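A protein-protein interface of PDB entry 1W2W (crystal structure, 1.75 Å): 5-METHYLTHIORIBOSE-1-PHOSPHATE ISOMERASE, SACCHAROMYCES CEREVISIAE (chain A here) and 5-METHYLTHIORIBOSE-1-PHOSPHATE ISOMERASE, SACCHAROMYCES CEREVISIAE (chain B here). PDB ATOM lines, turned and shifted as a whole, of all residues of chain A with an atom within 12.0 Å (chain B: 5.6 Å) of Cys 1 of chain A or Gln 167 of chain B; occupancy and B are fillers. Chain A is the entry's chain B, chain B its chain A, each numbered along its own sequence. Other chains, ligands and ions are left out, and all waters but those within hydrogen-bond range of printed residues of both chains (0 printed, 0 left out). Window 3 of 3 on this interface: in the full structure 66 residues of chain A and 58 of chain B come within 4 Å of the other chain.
The side-chain amide oxygen (OE1) of Gln 167 of chain B is in hydrogen-bond range of the side-chain sulfur (SG) of Cys 1 of chain A.
O of Asp 173 of chain B lies within hydrogen-bond range of N of Arg 3 of chain A.
NZ of Lys 208 of chain B lies within hydrogen-bond range of O of Pro 2 of chain A (2.8 Å).
The backbone carbonyl oxygen of Cys 1 of chain A sits close to the backbone carbonyl oxygen of Lys 172 of chain B (3.2 Å).
N of Phe 171 of chain B is in hydrogen-bond range of O of Leu 166 of chain B (3.0 Å).
The side-chain amino group of Lys 172 of chain B lies within hydrogen-bond range of the backbone carbonyl oxygen of Gly 170 of chain B (3.2 Å).
Cys 1 of chain A touches just these residues of chain B: Gln 167 (3.5 Å), Lys 172 (3.2 Å) and Lys 208 (3.9 Å).
Printed residues of chain B within 4 Å of Pro 2 of chain A: Ile 163 (3.8 Å), Gln 167 (3.7 Å), Phe 171 (3.4 Å), Lys 172 (3.6 Å), Asp 173 (3.2 Å) and Lys 208 (2.8 Å).
Of the printed residues of chain B, Arg 3 of chain A touches Asp 173 and Lys 208.
Pro 51 of chain A touches none of the printed residues of chain B.
Lys 87 of chain A touches none of the printed residues of chain B.
Printed residues of chain A within 4 Å of Leu 162 of chain B: Ala 54.
Ile 163 of chain B touches just one residue of chain A: Pro 2.
No residue of chain A comes within 4 Å of Asp 164 of chain B.
Val 165 of chain B touches none of the printed residues of chain A.
Gln 167 of chain B touches two residues of chain A.
No residue of chain A comes within 4 Å of Asp 169 of chain B.
Of chain A, only Cys 1 and Pro 2 come within 4 Å of Lys 172 of chain B.
Of the printed residues of chain A, Lys 208 of chain B touches Cys 1 (3.9 Å), Pro 2 (2.8 Å) and Arg 3 (3.9 Å).
The nearest residue of chain A that does not touch Gln 167 of chain B is Arg 3 of chain A (7.3 Å).
Of the 12 printed residues of chain A, 5 touch a printed residue of chain B.
Printed residues of chain A that touch a printed residue of chain B: Cys 1, Pro 2, Arg 3, Lys 53 and Ala 54.
Hydrophobic or aromatic side chains of chain A that line the printed part of chain B: Pro 2 and Ala 54.
Among the printed residues, 14 pairs touch across the chains.
Among the printed residues, no Asp or Glu carboxylate lies within 4 Å of a Lys or Arg side-chain nitrogen of the other chain.
Among the printed residues, pairs that only touch across the chains: Cys 1 of chain A with Lys 208 of chain B (3.9 Å), Pro 2 of chain A with Ile 163 of chain B (3.8 Å), Pro 2 of chain A with Gln 167 of chain B (3.7 Å), Pro 2 of chain A with Phe 171 of chain B (3.4 Å), Pro 2 of chain A with Lys 172 of chain B (3.6 Å), Pro 2 of chain A with Asp 173 of chain B (3.2 Å), Arg 3 of chain A with Lys 208 of chain B (3.9 Å), Lys 53 of chain A with Leu 166 of chain B (3.7 Å), Lys 53 of chain A with Phe 171 of chain B (3.4 Å) and Ala 54 of chain A with Leu 162 of chain B (3.8 Å).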
ATOM      1  N   CYS A   1       9.341 -10.185  31.366  1.00  0.00           N
ATOM      2  CA  CYS A   1       8.836  -8.978  30.662  1.00  0.00           C
ATOM      3  C   CYS A   1       9.975  -7.967  30.631  1.00  0.00           C
ATOM      4  O   CYS A   1      10.777  -7.911  31.565  1.00  0.00           O
ATOM      5  CB  CYS A   1       7.634  -8.380  31.403  1.00  0.00           C
ATOM      6  SG  CYS A   1       6.049  -9.221  31.112  1.00  0.00           S
ATOM      7  N   PRO A   2      10.046  -7.175  29.568  1.00  0.00           N
ATOM      8  CA  PRO A   2      11.086  -6.146  29.459  1.00  0.00           C
ATOM      9  C   PRO A   2      10.844  -5.029  30.465  1.00  0.00           C
ATOM     10  O   PRO A   2       9.708  -4.777  30.860  1.00  0.00           O
ATOM     11  CB  PRO A   2      10.928  -5.634  28.030  1.00  0.00           C
ATOM     12  CG  PRO A   2       9.526  -5.929  27.669  1.00  0.00           C
ATOM     13  CD  PRO A   2       9.157  -7.189  28.395  1.00  0.00           C
ATOM     14  N   ARG A   3      11.914  -4.367  30.880  1.00  0.00           N
ATOM     15  CA  ARG A   3      11.788  -3.269  31.828  1.00  0.00           C
ATOM     16  C   ARG A   3      12.998  -2.391  31.625  1.00  0.00           C
ATOM     17  O   ARG A   3      14.067  -2.889  31.270  1.00  0.00           O
ATOM     18  CB  ARG A   3      11.746  -3.784  33.269  1.00  0.00           C
ATOM     19  CG  ARG A   3      13.050  -4.423  33.741  1.00  0.00           C
ATOM     20  CD  ARG A   3      12.951  -5.111  35.100  1.00  0.00           C
ATOM     21  NE  ARG A   3      14.275  -5.362  35.665  1.00  0.00           N
ATOM     22  CZ  ARG A   3      15.029  -6.423  35.386  1.00  0.00           C
ATOM     23  NH1 ARG A   3      14.600  -7.360  34.543  1.00  0.00           N
ATOM     24  NH2 ARG A   3      16.219  -6.550  35.955  1.00  0.00           N
ATOM     25  N   MET A   4      12.816  -1.092  31.841  1.00  0.00           N
ATOM     26  CA  MET A   4      13.932  -0.161  31.758  1.00  0.00           C
ATOM     27  C   MET A   4      14.824  -0.282  32.973  1.00  0.00           C
ATOM     28  O   MET A   4      14.366  -0.107  34.112  1.00  0.00           O
ATOM     29  CB  MET A   4      13.423   1.277  31.699  1.00  0.00           C
ATOM     30  CG  MET A   4      14.525   2.245  31.345  1.00  0.00           C
ATOM     31  SD  MET A   4      13.893   4.067  31.487  1.00  0.00           S
ATOM     32  CE  MET A   4      13.703   4.160  33.452  1.00  0.00           C
ATOM     33  N   GLY A   5      16.102  -0.560  32.738  1.00  0.00           N
ATOM     34  CA  GLY A   5      17.031  -0.697  33.842  1.00  0.00           C
ATOM     35  C   GLY A   5      18.062   0.413  33.918  1.00  0.00           C
ATOM     36  O   GLY A   5      18.802   0.494  34.895  1.00  0.00           O
ATOM     37  N   HIS A   6      18.126   1.279  32.908  1.00  0.00           N
ATOM     38  CA  HIS A   6      19.128   2.344  32.959  1.00  0.00           C
ATOM     39  C   HIS A   6      18.790   3.488  32.025  1.00  0.00           C
ATOM     40  O   HIS A   6      18.143   3.289  30.994  1.00  0.00           O
ATOM     41  CB  HIS A   6      20.508   1.775  32.576  1.00  0.00           C
ATOM     42  CG  HIS A   6      21.648   2.397  33.327  1.00  0.00           C
ATOM     43  ND1 HIS A   6      22.042   1.960  34.575  1.00  0.00           N
ATOM     44  CD2 HIS A   6      22.481   3.417  33.006  1.00  0.00           C
ATOM     45  CE1 HIS A   6      23.069   2.682  34.989  1.00  0.00           C
ATOM     46  NE2 HIS A   6      23.353   3.574  34.057  1.00  0.00           N
ATOM     47  N   ILE A  50      23.615  -3.116  28.592  1.00  0.00           N
ATOM     48  CA  ILE A  50      22.164  -3.232  28.622  1.00  0.00           C
ATOM     49  C   ILE A  50      21.747  -2.628  27.273  1.00  0.00           C
ATOM     50  O   ILE A  50      22.090  -1.476  27.000  1.00  0.00           O
ATOM     51  CB  ILE A  50      21.643  -2.345  29.799  1.00  0.00           C
ATOM     52  CG1 ILE A  50      22.230  -2.820  31.134  1.00  0.00           C
ATOM     53  CG2 ILE A  50      20.127  -2.284  29.836  1.00  0.00           C
ATOM     54  CD1 ILE A  50      21.586  -2.192  32.389  1.00  0.00           C
ATOM     55  N   PRO A  51      21.032  -3.369  26.427  1.00  0.00           N
ATOM     56  CA  PRO A  51      20.738  -2.894  25.065  1.00  0.00           C
ATOM     57  C   PRO A  51      19.942  -1.586  25.121  1.00  0.00           C
ATOM     58  O   PRO A  51      18.985  -1.490  25.892  1.00  0.00           O
ATOM     59  CB  PRO A  51      19.845  -3.995  24.486  1.00  0.00           C
ATOM     60  CG  PRO A  51      20.088  -5.202  25.342  1.00  0.00           C
ATOM     61  CD  PRO A  51      20.465  -4.701  26.701  1.00  0.00           C
ATOM     62  N   LYS A  53      17.181   0.662  23.740  1.00  0.00           N
ATOM     63  CA  LYS A  53      16.031   0.327  22.909  1.00  0.00           C
ATOM     64  C   LYS A  53      15.192   1.528  22.482  1.00  0.00           C
ATOM     65  O   LYS A  53      14.270   1.382  21.675  1.00  0.00           O
ATOM     66  CB  LYS A  53      15.146  -0.696  23.625  1.00  0.00           C
ATOM     67  CG  LYS A  53      15.791  -2.075  23.689  1.00  0.00           C
ATOM     68  CD  LYS A  53      15.566  -2.782  22.352  1.00  0.00           C
ATOM     69  CE  LYS A  53      16.423  -4.022  22.223  1.00  0.00           C
ATOM     70  NZ  LYS A  53      16.186  -4.659  20.898  1.00  0.00           N
ATOM     71  N   ALA A  54      15.501   2.700  23.019  1.00  0.00           N
ATOM     72  CA  ALA A  54      14.795   3.906  22.611  1.00  0.00           C
ATOM     73  C   ALA A  54      15.570   5.155  23.000  1.00  0.00           C
ATOM     74  O   ALA A  54      16.323   5.160  23.979  1.00  0.00           O
ATOM     75  CB  ALA A  54      13.383   3.951  23.199  1.00  0.00           C
ATOM     76  N   LYS A  87      14.677   2.999  18.055  1.00  0.00           N
ATOM     77  CA  LYS A  87      13.487   3.836  17.914  1.00  0.00           C
ATOM     78  C   LYS A  87      13.717   5.217  18.523  1.00  0.00           C
ATOM     79  O   LYS A  87      14.281   5.331  19.606  1.00  0.00           O
ATOM     80  CB  LYS A  87      12.288   3.172  18.587  1.00  0.00           C
ATOM     81  CG  LYS A  87      11.822   1.909  17.879  1.00  0.00           C
ATOM     82  CD  LYS A  87      10.934   2.236  16.702  1.00  0.00           C
ATOM     83  CE  LYS A  87      10.177   0.995  16.213  1.00  0.00           C
ATOM     84  NZ  LYS A  87      11.137  -0.117  15.969  1.00  0.00           N
ATOM     85  N   PHE A  89      11.791   8.769  19.607  1.00  0.00           N
ATOM     86  CA  PHE A  89      10.483   9.354  19.900  1.00  0.00           C
ATOM     87  C   PHE A  89      10.587  10.784  20.410  1.00  0.00           C
ATOM     88  O   PHE A  89      11.392  11.087  21.281  1.00  0.00           O
ATOM     89  CB  PHE A  89       9.782   8.524  20.967  1.00  0.00           C
ATOM     90  CG  PHE A  89       9.528   7.101  20.565  1.00  0.00           C
ATOM     91  CD1 PHE A  89       8.560   6.802  19.617  1.00  0.00           C
ATOM     92  CD2 PHE A  89      10.235   6.065  21.162  1.00  0.00           C
ATOM     93  CE1 PHE A  89       8.316   5.486  19.250  1.00  0.00           C
ATOM     94  CE2 PHE A  89       9.994   4.754  20.804  1.00  0.00           C
ATOM     95  CZ  PHE A  89       9.033   4.468  19.851  1.00  0.00           C
ATOM     96  N   LEU B 162       6.175   1.856  24.341  1.00  0.00           N
ATOM     97  CA  LEU B 162       7.460   1.177  24.193  1.00  0.00           C
ATOM     98  C   LEU B 162       7.412  -0.264  24.711  1.00  0.00           C
ATOM     99  O   LEU B 162       7.909  -1.182  24.046  1.00  0.00           O
ATOM    100  CB  LEU B 162       8.605   1.959  24.852  1.00  0.00           C
ATOM    101  CG  LEU B 162       9.999   1.329  24.728  1.00  0.00           C
ATOM    102  CD1 LEU B 162      10.426   1.241  23.268  1.00  0.00           C
ATOM    103  CD2 LEU B 162      11.021   2.162  25.539  1.00  0.00           C
ATOM    104  N   ILE B 163       6.812  -0.471  25.878  1.00  0.00           N
ATOM    105  CA  ILE B 163       6.707  -1.826  26.418  1.00  0.00           C
ATOM    106  C   ILE B 163       5.967  -2.736  25.446  1.00  0.00           C
ATOM    107  O   ILE B 163       6.378  -3.876  25.224  1.00  0.00           O
ATOM    108  CB  ILE B 163       6.058  -1.825  27.806  1.00  0.00           C
ATOM    109  CG1 ILE B 163       6.965  -1.106  28.804  1.00  0.00           C
ATOM    110  CG2 ILE B 163       5.722  -3.261  28.270  1.00  0.00           C
ATOM    111  CD1 ILE B 163       8.360  -1.708  28.980  1.00  0.00           C
ATOM    112  N   ASP B 164       4.890  -2.226  24.854  1.00  0.00           N
ATOM    113  CA  ASP B 164       4.117  -2.993  23.878  1.00  0.00           C
ATOM    114  C   ASP B 164       4.919  -3.333  22.621  1.00  0.00           C
ATOM    115  O   ASP B 164       4.858  -4.466  22.123  1.00  0.00           O
ATOM    116  CB  ASP B 164       2.833  -2.255  23.481  1.00  0.00           C
ATOM    117  CG  ASP B 164       1.785  -2.235  24.587  1.00  0.00           C
ATOM    118  OD1 ASP B 164       1.866  -3.021  25.560  1.00  0.00           O
ATOM    119  OD2 ASP B 164       0.825  -1.438  24.554  1.00  0.00           O
ATOM    120  N   VAL B 165       5.674  -2.360  22.109  1.00  0.00           N
ATOM    121  CA  VAL B 165       6.569  -2.577  20.979  1.00  0.00           C
ATOM    122  C   VAL B 165       7.596  -3.682  21.270  1.00  0.00           C
ATOM    123  O   VAL B 165       7.822  -4.571  20.438  1.00  0.00           O
ATOM    124  CB  VAL B 165       7.308  -1.276  20.604  1.00  0.00           C
ATOM    125  CG1 VAL B 165       8.520  -1.576  19.737  1.00  0.00           C
ATOM    126  CG2 VAL B 165       6.346  -0.318  19.896  1.00  0.00           C
ATOM    127  N   LEU B 166       8.213  -3.610  22.448  1.00  0.00           N
ATOM    128  CA  LEU B 166       9.216  -4.596  22.851  1.00  0.00           C
ATOM    129  C   LEU B 166       8.587  -5.965  23.082  1.00  0.00           C
ATOM    130  O   LEU B 166       9.151  -6.991  22.709  1.00  0.00           O
ATOM    131  CB  LEU B 166       9.951  -4.125  24.107  1.00  0.00           C
ATOM    132  CG  LEU B 166      10.779  -2.854  23.919  1.00  0.00           C
ATOM    133  CD1 LEU B 166      11.325  -2.367  25.278  1.00  0.00           C
ATOM    134  CD2 LEU B 166      11.902  -3.056  22.908  1.00  0.00           C
ATOM    135  N   GLN B 167       7.415  -5.976  23.702  1.00  0.00           N
ATOM    136  CA  GLN B 167       6.705  -7.229  23.929  1.00  0.00           C
ATOM    137  C   GLN B 167       6.310  -7.883  22.605  1.00  0.00           C
ATOM    138  O   GLN B 167       6.434  -9.104  22.462  1.00  0.00           O
ATOM    139  CB  GLN B 167       5.557  -7.075  24.945  1.00  0.00           C
ATOM    140  CG  GLN B 167       6.061  -7.145  26.401  1.00  0.00           C
ATOM    141  CD  GLN B 167       5.055  -6.798  27.498  1.00  0.00           C
ATOM    142  OE1 GLN B 167       5.401  -6.843  28.692  1.00  0.00           O
ATOM    143  NE2 GLN B 167       3.827  -6.454  27.115  1.00  0.00           N
ATOM    144  N   LYS B 168       5.875  -7.089  21.628  1.00  0.00           N
ATOM    145  CA  LYS B 168       5.637  -7.625  20.289  1.00  0.00           C
ATOM    146  C   LYS B 168       6.879  -8.218  19.616  1.00  0.00           C
ATOM    147  O   LYS B 168       6.794  -9.256  18.946  1.00  0.00           O
ATOM    148  CB  LYS B 168       4.993  -6.587  19.367  1.00  0.00           C
ATOM    149  CG  LYS B 168       4.517  -7.186  18.058  1.00  0.00           C
ATOM    150  CD  LYS B 168       3.900  -6.149  17.127  1.00  0.00           C
ATOM    151  CE  LYS B 168       3.798  -6.711  15.713  1.00  0.00           C
ATOM    152  NZ  LYS B 168       2.848  -5.962  14.854  1.00  0.00           N
ATOM    153  N   ASP B 169       8.024  -7.558  19.786  1.00  0.00           N
ATOM    154  CA  ASP B 169       9.287  -8.008  19.208  1.00  0.00           C
ATOM    155  C   ASP B 169       9.938  -9.163  19.974  1.00  0.00           C
ATOM    156  O   ASP B 169      11.002  -9.649  19.587  1.00  0.00           O
ATOM    157  CB  ASP B 169      10.270  -6.839  19.078  1.00  0.00           C
ATOM    158  CG  ASP B 169       9.861  -5.845  17.995  1.00  0.00           C
ATOM    159  OD1 ASP B 169       8.938  -6.153  17.210  1.00  0.00           O
ATOM    160  OD2 ASP B 169      10.402  -4.726  17.843  1.00  0.00           O
ATOM    161  N   GLY B 170       9.304  -9.597  21.058  1.00  0.00           N
ATOM    162  CA  GLY B 170       9.815 -10.676  21.883  1.00  0.00           C
ATOM    163  C   GLY B 170      11.075 -10.338  22.664  1.00  0.00           C
ATOM    164  O   GLY B 170      11.829 -11.228  23.063  1.00  0.00           O
ATOM    165  N   PHE B 171      11.307  -9.048  22.890  1.00  0.00           N
ATOM    166  CA  PHE B 171      12.352  -8.608  23.805  1.00  0.00           C
ATOM    167  C   PHE B 171      11.887  -8.752  25.248  1.00  0.00           C
ATOM    168  O   PHE B 171      10.828  -8.246  25.616  1.00  0.00           O
ATOM    169  CB  PHE B 171      12.724  -7.154  23.522  1.00  0.00           C
ATOM    170  CG  PHE B 171      13.918  -6.687  24.293  1.00  0.00           C
ATOM    171  CD1 PHE B 171      15.198  -6.969  23.845  1.00  0.00           C
ATOM    172  CD2 PHE B 171      13.765  -5.974  25.468  1.00  0.00           C
ATOM    173  CE1 PHE B 171      16.307  -6.535  24.566  1.00  0.00           C
ATOM    174  CE2 PHE B 171      14.863  -5.546  26.188  1.00  0.00           C
ATOM    175  CZ  PHE B 171      16.130  -5.823  25.739  1.00  0.00           C
ATOM    176  N   LYS B 172      12.668  -9.441  26.067  1.00  0.00           N
ATOM    177  CA  LYS B 172      12.192  -9.806  27.397  1.00  0.00           C
ATOM    178  C   LYS B 172      13.090  -9.300  28.522  1.00  0.00           C
ATOM    179  O   LYS B 172      12.796  -9.492  29.706  1.00  0.00           O
ATOM    180  CB  LYS B 172      11.964 -11.321  27.488  1.00  0.00           C
ATOM    181  CG  LYS B 172      10.701 -11.765  26.762  1.00  0.00           C
ATOM    182  CD  LYS B 172      10.717 -13.247  26.389  1.00  0.00           C
ATOM    183  CE  LYS B 172      10.039 -13.488  25.040  1.00  0.00           C
ATOM    184  NZ  LYS B 172      10.946 -14.133  24.036  1.00  0.00           N
ATOM    185  N   ASP B 173      14.177  -8.638  28.148  1.00  0.00           N
ATOM    186  CA  ASP B 173      15.232  -8.315  29.096  1.00  0.00           C
ATOM    187  C   ASP B 173      15.185  -6.880  29.642  1.00  0.00           C
ATOM    188  O   ASP B 173      14.304  -6.096  29.289  1.00  0.00           O
ATOM    189  CB  ASP B 173      16.591  -8.648  28.467  1.00  0.00           C
ATOM    190  CG  ASP B 173      16.670 -10.099  28.005  1.00  0.00           C
ATOM    191  OD1 ASP B 173      16.301 -10.979  28.810  1.00  0.00           O
ATOM    192  OD2 ASP B 173      17.072 -10.456  26.872  1.00  0.00           O
ATOM    193  N   LYS B 208       7.987  -4.433  38.562  1.00  0.00           N
ATOM    194  CA  LYS B 208       8.461  -5.738  38.105  1.00  0.00           C
ATOM    195  C   LYS B 208       9.552  -6.343  38.995  1.00  0.00           C
ATOM    196  O   LYS B 208       9.507  -7.536  39.304  1.00  0.00           O
ATOM    197  CB  LYS B 208       8.886  -5.694  36.633  1.00  0.00           C
ATOM    198  CG  LYS B 208       7.712  -5.526  35.665  1.00  0.00           C
ATOM    199  CD  LYS B 208       8.139  -4.997  34.299  1.00  0.00           C
ATOM    200  CE  LYS B 208       6.969  -5.016  33.308  1.00  0.00           C
ATOM    201  NZ  LYS B 208       7.219  -4.269  32.029  1.00  0.00           N
